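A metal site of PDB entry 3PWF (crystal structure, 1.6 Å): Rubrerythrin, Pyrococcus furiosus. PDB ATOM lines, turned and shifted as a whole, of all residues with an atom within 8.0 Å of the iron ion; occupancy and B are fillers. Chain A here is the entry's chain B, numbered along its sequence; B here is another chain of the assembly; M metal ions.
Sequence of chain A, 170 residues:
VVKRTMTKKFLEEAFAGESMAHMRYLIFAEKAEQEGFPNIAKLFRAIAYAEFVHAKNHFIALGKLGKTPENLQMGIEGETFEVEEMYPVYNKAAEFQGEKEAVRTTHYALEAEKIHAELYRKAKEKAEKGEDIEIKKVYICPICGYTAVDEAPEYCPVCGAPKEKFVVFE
N of Cys 156 is in hydrogen-bond range of O of Ala 161.
N of Cys 141 is in hydrogen-bond range of O of Tyr 146 (2.8 Å).
N of Val 158 sits close to SG of Cys 156.
The side-chain sulfur (SG) of Cys 159 lies close to the backbone NH (N) of Ala 161, 3.6 Å away.
The backbone NH (N) of Ile 143 sits close to the side-chain sulfur (SG) of Cys 141, at 3.5 Å.
The side-chain sulfur of Cys 144 sits close to the backbone NH of Tyr 146 (3.4 Å).
Four residues have an atom within 4 Å of the iron ion: Cys 141, Cys 144, Cys 156 and Cys 159.
The nearest printed residue that does not touch the iron ion is Tyr 146 (4.2 Å).
SG of Cys 144 binds the iron ion, at 2.3 Å.
The iron ion is bound by the side-chain sulfur (SG) of Cys 159 (2.3 Å).
The iron ion is bound by the side-chain sulfur (SG) of Cys 156 (2.4 Å).
SG of Cys 141 binds the iron ion (2.4 Å).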
ATOM      1  N   TYR A 108     -12.530 -19.652  -4.638  1.00  0.00           N
ATOM      2  CA  TYR A 108     -11.095 -19.935  -4.825  1.00  0.00           C
ATOM      3  C   TYR A 108     -10.927 -21.204  -5.585  1.00  0.00           C
ATOM      4  O   TYR A 108     -10.137 -21.289  -6.519  1.00  0.00           O
ATOM      5  CB  TYR A 108     -10.468 -20.093  -3.400  1.00  0.00           C
ATOM      6  CG  TYR A 108     -10.201 -18.805  -2.658  1.00  0.00           C
ATOM      7  CD1 TYR A 108     -10.404 -17.552  -3.237  1.00  0.00           C
ATOM      8  CD2 TYR A 108      -9.683 -18.876  -1.409  1.00  0.00           C
ATOM      9  CE1 TYR A 108      -9.997 -16.370  -2.522  1.00  0.00           C
ATOM     10  CE2 TYR A 108      -9.311 -17.733  -0.662  1.00  0.00           C
ATOM     11  CZ  TYR A 108      -9.445 -16.483  -1.312  1.00  0.00           C
ATOM     12  OH  TYR A 108      -9.020 -15.360  -0.557  1.00  0.00           O
ATOM     13  N   ILE A 140       2.053 -22.244  -7.703  1.00  0.00           N
ATOM     14  CA  ILE A 140       0.714 -22.415  -7.077  1.00  0.00           C
ATOM     15  C   ILE A 140       0.562 -21.423  -5.925  1.00  0.00           C
ATOM     16  O   ILE A 140       1.467 -21.270  -5.054  1.00  0.00           O
ATOM     17  CB  ILE A 140       0.611 -23.831  -6.432  1.00  0.00           C
ATOM     18  CG1 ILE A 140       0.940 -24.965  -7.493  1.00  0.00           C
ATOM     19  CG2 ILE A 140      -0.832 -24.017  -5.813  1.00  0.00           C
ATOM     20  CD1 ILE A 140      -0.091 -25.075  -8.653  1.00  0.00           C
ATOM     21  N   CYS A 141      -0.590 -20.701  -5.871  1.00  0.00           N
ATOM     22  CA  CYS A 141      -0.823 -19.764  -4.777  1.00  0.00           C
ATOM     23  C   CYS A 141      -1.168 -20.559  -3.504  1.00  0.00           C
ATOM     24  O   CYS A 141      -2.086 -21.378  -3.556  1.00  0.00           O
ATOM     25  CB  CYS A 141      -1.990 -18.810  -5.153  1.00  0.00           C
ATOM     26  SG  CYS A 141      -2.353 -17.706  -3.820  1.00  0.00           S
ATOM     27  N   PRO A 142      -0.443 -20.327  -2.389  1.00  0.00           N
ATOM     28  CA  PRO A 142      -0.750 -21.088  -1.136  1.00  0.00           C
ATOM     29  C   PRO A 142      -2.032 -20.616  -0.440  1.00  0.00           C
ATOM     30  O   PRO A 142      -2.440 -21.255   0.552  1.00  0.00           O
ATOM     31  CB  PRO A 142       0.482 -20.829  -0.251  1.00  0.00           C
ATOM     32  CG  PRO A 142       0.945 -19.370  -0.734  1.00  0.00           C
ATOM     33  CD  PRO A 142       0.737 -19.419  -2.286  1.00  0.00           C
ATOM     34  N   ILE A 143      -2.601 -19.481  -0.841  1.00  0.00           N
ATOM     35  CA  ILE A 143      -3.883 -18.945  -0.301  1.00  0.00           C
ATOM     36  C   ILE A 143      -5.059 -19.545  -0.973  1.00  0.00           C
ATOM     37  O   ILE A 143      -6.005 -19.936  -0.269  1.00  0.00           O
ATOM     38  CB  ILE A 143      -3.920 -17.405  -0.474  1.00  0.00           C
ATOM     39  CG1 ILE A 143      -2.607 -16.788   0.028  1.00  0.00           C
ATOM     40  CG2 ILE A 143      -5.240 -16.827   0.179  1.00  0.00           C
ATOM     41  CD1 ILE A 143      -2.120 -17.188   1.255  1.00  0.00           C
ATOM     42  N   CYS A 144      -5.100 -19.600  -2.320  1.00  0.00           N
ATOM     43  CA  CYS A 144      -6.273 -19.975  -3.010  1.00  0.00           C
ATOM     44  C   CYS A 144      -6.124 -21.219  -3.946  1.00  0.00           C
ATOM     45  O   CYS A 144      -7.110 -21.666  -4.590  1.00  0.00           O
ATOM     46  CB  CYS A 144      -7.036 -18.794  -3.703  1.00  0.00           C
ATOM     47  SG  CYS A 144      -5.955 -18.270  -5.138  1.00  0.00           S
ATOM     48  N   GLY A 145      -4.846 -21.561  -4.202  1.00  0.00           N
ATOM     49  CA  GLY A 145      -4.587 -22.602  -5.158  1.00  0.00           C
ATOM     50  C   GLY A 145      -4.601 -22.198  -6.608  1.00  0.00           C
ATOM     51  O   GLY A 145      -4.417 -23.057  -7.465  1.00  0.00           O
ATOM     52  N   TYR A 146      -4.608 -20.877  -6.931  1.00  0.00           N
ATOM     53  CA  TYR A 146      -4.438 -20.496  -8.286  1.00  0.00           C
ATOM     54  C   TYR A 146      -3.156 -21.066  -8.858  1.00  0.00           C
ATOM     55  O   TYR A 146      -2.113 -21.146  -8.193  1.00  0.00           O
ATOM     56  CB  TYR A 146      -4.351 -18.934  -8.243  1.00  0.00           C
ATOM     57  CG  TYR A 146      -4.404 -18.412  -9.700  1.00  0.00           C
ATOM     58  CD1 TYR A 146      -5.586 -18.495 -10.357  1.00  0.00           C
ATOM     59  CD2 TYR A 146      -3.336 -17.995 -10.283  1.00  0.00           C
ATOM     60  CE1 TYR A 146      -5.671 -18.094 -11.681  1.00  0.00           C
ATOM     61  CE2 TYR A 146      -3.386 -17.570 -11.688  1.00  0.00           C
ATOM     62  CZ  TYR A 146      -4.541 -17.623 -12.291  1.00  0.00           C
ATOM     63  OH  TYR A 146      -4.676 -17.208 -13.610  1.00  0.00           O
ATOM     64  N   THR A 147      -3.221 -21.465 -10.138  1.00  0.00           N
ATOM     65  CA  THR A 147      -2.175 -22.251 -10.698  1.00  0.00           C
ATOM     66  C   THR A 147      -1.717 -21.556 -12.011  1.00  0.00           C
ATOM     67  O   THR A 147      -2.541 -21.157 -12.845  1.00  0.00           O
ATOM     68  CB  THR A 147      -2.808 -23.606 -11.069  1.00  0.00           C
ATOM     69  OG1 THR A 147      -3.225 -24.267  -9.850  1.00  0.00           O
ATOM     70  CG2 THR A 147      -1.752 -24.551 -11.746  1.00  0.00           C
ATOM     71  N   PRO A 153       2.087 -14.775 -11.942  1.00  0.00           N
ATOM     72  CA  PRO A 153       1.522 -13.465 -12.336  1.00  0.00           C
ATOM     73  C   PRO A 153       2.049 -12.445 -11.337  1.00  0.00           C
ATOM     74  O   PRO A 153       2.478 -12.802 -10.282  1.00  0.00           O
ATOM     75  CB  PRO A 153      -0.050 -13.704 -12.196  1.00  0.00           C
ATOM     76  CG  PRO A 153      -0.186 -14.768 -11.127  1.00  0.00           C
ATOM     77  CD  PRO A 153       1.082 -15.708 -11.341  1.00  0.00           C
ATOM     78  N   TYR A 155       0.504 -10.554  -9.394  1.00  0.00           N
ATOM     79  CA  TYR A 155      -0.271 -10.844  -8.153  1.00  0.00           C
ATOM     80  C   TYR A 155      -1.306 -11.855  -8.598  1.00  0.00           C
ATOM     81  O   TYR A 155      -1.673 -11.971  -9.785  1.00  0.00           O
ATOM     82  CB  TYR A 155      -0.946  -9.539  -7.603  1.00  0.00           C
ATOM     83  CG  TYR A 155      -2.021  -8.886  -8.470  1.00  0.00           C
ATOM     84  CD1 TYR A 155      -3.357  -9.324  -8.420  1.00  0.00           C
ATOM     85  CD2 TYR A 155      -1.729  -7.809  -9.361  1.00  0.00           C
ATOM     86  CE1 TYR A 155      -4.391  -8.807  -9.233  1.00  0.00           C
ATOM     87  CE2 TYR A 155      -2.750  -7.282 -10.124  1.00  0.00           C
ATOM     88  CZ  TYR A 155      -4.099  -7.726 -10.115  1.00  0.00           C
ATOM     89  OH  TYR A 155      -5.206  -7.212 -10.907  1.00  0.00           O
ATOM     90  N   CYS A 156      -1.790 -12.643  -7.572  1.00  0.00           N
ATOM     91  CA  CYS A 156      -2.801 -13.664  -7.939  1.00  0.00           C
ATOM     92  C   CYS A 156      -4.142 -12.955  -8.263  1.00  0.00           C
ATOM     93  O   CYS A 156      -4.636 -12.146  -7.447  1.00  0.00           O
ATOM     94  CB  CYS A 156      -2.978 -14.296  -6.610  1.00  0.00           C
ATOM     95  SG  CYS A 156      -4.256 -15.702  -6.809  1.00  0.00           S
ATOM     96  N   PRO A 157      -4.748 -13.285  -9.355  1.00  0.00           N
ATOM     97  CA  PRO A 157      -5.945 -12.606  -9.761  1.00  0.00           C
ATOM     98  C   PRO A 157      -7.122 -12.987  -8.950  1.00  0.00           C
ATOM     99  O   PRO A 157      -8.148 -12.261  -8.916  1.00  0.00           O
ATOM    100  CB  PRO A 157      -6.124 -13.031 -11.277  1.00  0.00           C
ATOM    101  CG  PRO A 157      -5.313 -14.317 -11.326  1.00  0.00           C
ATOM    102  CD  PRO A 157      -4.206 -14.184 -10.372  1.00  0.00           C
ATOM    103  N   VAL A 158      -6.967 -14.106  -8.205  1.00  0.00           N
ATOM    104  CA  VAL A 158      -8.121 -14.573  -7.408  1.00  0.00           C
ATOM    105  C   VAL A 158      -8.126 -14.013  -5.959  1.00  0.00           C
ATOM    106  O   VAL A 158      -9.189 -13.594  -5.451  1.00  0.00           O
ATOM    107  CB  VAL A 158      -8.124 -16.140  -7.405  1.00  0.00           C
ATOM    108  CG1 VAL A 158      -9.353 -16.692  -6.520  1.00  0.00           C
ATOM    109  CG2 VAL A 158      -8.282 -16.663  -8.901  1.00  0.00           C
ATOM    110  N   CYS A 159      -6.966 -14.001  -5.280  1.00  0.00           N
ATOM    111  CA  CYS A 159      -6.974 -13.557  -3.899  1.00  0.00           C
ATOM    112  C   CYS A 159      -6.125 -12.292  -3.685  1.00  0.00           C
ATOM    113  O   CYS A 159      -6.113 -11.740  -2.601  1.00  0.00           O
ATOM    114  CB  CYS A 159      -6.452 -14.686  -2.924  1.00  0.00           C
ATOM    115  SG  CYS A 159      -4.722 -15.041  -3.072  1.00  0.00           S
ATOM    116  N   GLY A 160      -5.327 -11.910  -4.672  1.00  0.00           N
ATOM    117  CA  GLY A 160      -4.509 -10.657  -4.486  1.00  0.00           C
ATOM    118  C   GLY A 160      -3.104 -10.937  -4.055  1.00  0.00           C
ATOM    119  O   GLY A 160      -2.261  -9.985  -3.984  1.00  0.00           O
ATOM    120  N   ALA A 161      -2.712 -12.154  -3.695  1.00  0.00           N
ATOM    121  CA  ALA A 161      -1.411 -12.333  -3.131  1.00  0.00           C
ATOM    122  C   ALA A 161      -0.279 -11.989  -4.099  1.00  0.00           C
ATOM    123  O   ALA A 161      -0.363 -12.233  -5.261  1.00  0.00           O
ATOM    124  CB  ALA A 161      -1.208 -13.932  -2.768  1.00  0.00           C
ATOM    125  N   PRO A 162       0.818 -11.439  -3.538  1.00  0.00           N
ATOM    126  CA  PRO A 162       1.903 -11.078  -4.460  1.00  0.00           C
ATOM    127  C   PRO A 162       2.623 -12.318  -5.051  1.00  0.00           C
ATOM    128  O   PRO A 162       2.707 -13.358  -4.353  1.00  0.00           O
ATOM    129  CB  PRO A 162       2.881 -10.256  -3.569  1.00  0.00           C
ATOM    130  CG  PRO A 162       2.558 -10.543  -2.173  1.00  0.00           C
ATOM    131  CD  PRO A 162       1.033 -11.081  -2.137  1.00  0.00           C
ATOM    132  N   LYS A 165       4.705 -14.900  -2.999  1.00  0.00           N
ATOM    133  CA  LYS A 165       4.221 -16.000  -2.157  1.00  0.00           C
ATOM    134  C   LYS A 165       3.905 -17.195  -2.897  1.00  0.00           C
ATOM    135  O   LYS A 165       3.673 -18.183  -2.201  1.00  0.00           O
ATOM    136  CB  LYS A 165       3.078 -15.764  -1.288  1.00  0.00           C
ATOM    137  CG  LYS A 165       2.302 -14.768  -1.618  1.00  0.00           C
ATOM    138  CD  LYS A 165       2.644 -13.794  -0.503  1.00  0.00           C
ATOM    139  CE  LYS A 165       3.253 -14.429   0.748  1.00  0.00           C
ATOM    140  NZ  LYS A 165       3.825 -13.281   1.550  1.00  0.00           N
ATOM    141  N   PHE A 166       3.949 -17.162  -4.228  1.00  0.00           N
ATOM    142  CA  PHE A 166       3.647 -18.455  -4.905  1.00  0.00           C
ATOM    143  C   PHE A 166       4.704 -19.546  -4.551  1.00  0.00           C
ATOM    144  O   PHE A 166       5.913 -19.304  -4.426  1.00  0.00           O
ATOM    145  CB  PHE A 166       3.596 -18.291  -6.406  1.00  0.00           C
ATOM    146  CG  PHE A 166       2.283 -17.634  -6.964  1.00  0.00           C
ATOM    147  CD1 PHE A 166       1.375 -18.441  -7.660  1.00  0.00           C
ATOM    148  CD2 PHE A 166       1.856 -16.360  -6.641  1.00  0.00           C
ATOM    149  CE1 PHE A 166       0.099 -17.920  -8.090  1.00  0.00           C
ATOM    150  CE2 PHE A 166       0.676 -15.740  -7.216  1.00  0.00           C
ATOM    151  CZ  PHE A 166      -0.233 -16.577  -7.934  1.00  0.00           C
ATOM    152  N   VAL B  53      -4.458 -26.998  -1.017  1.00  0.00           N
ATOM    153  CA  VAL B  53      -4.899 -25.646  -0.540  1.00  0.00           C
ATOM    154  C   VAL B  53      -6.424 -25.552  -0.495  1.00  0.00           C
ATOM    155  O   VAL B  53      -7.022 -25.073   0.507  1.00  0.00           O
ATOM    156  CB  VAL B  53      -4.338 -24.604  -1.489  1.00  0.00           C
ATOM    157  CG1 VAL B  53      -4.848 -23.203  -1.050  1.00  0.00           C
ATOM    158  CG2 VAL B  53      -2.759 -24.618  -1.433  1.00  0.00           C
HETATM  159 FE    FE M   1      -4.333 -16.704  -4.679  1.00  0.00          FE
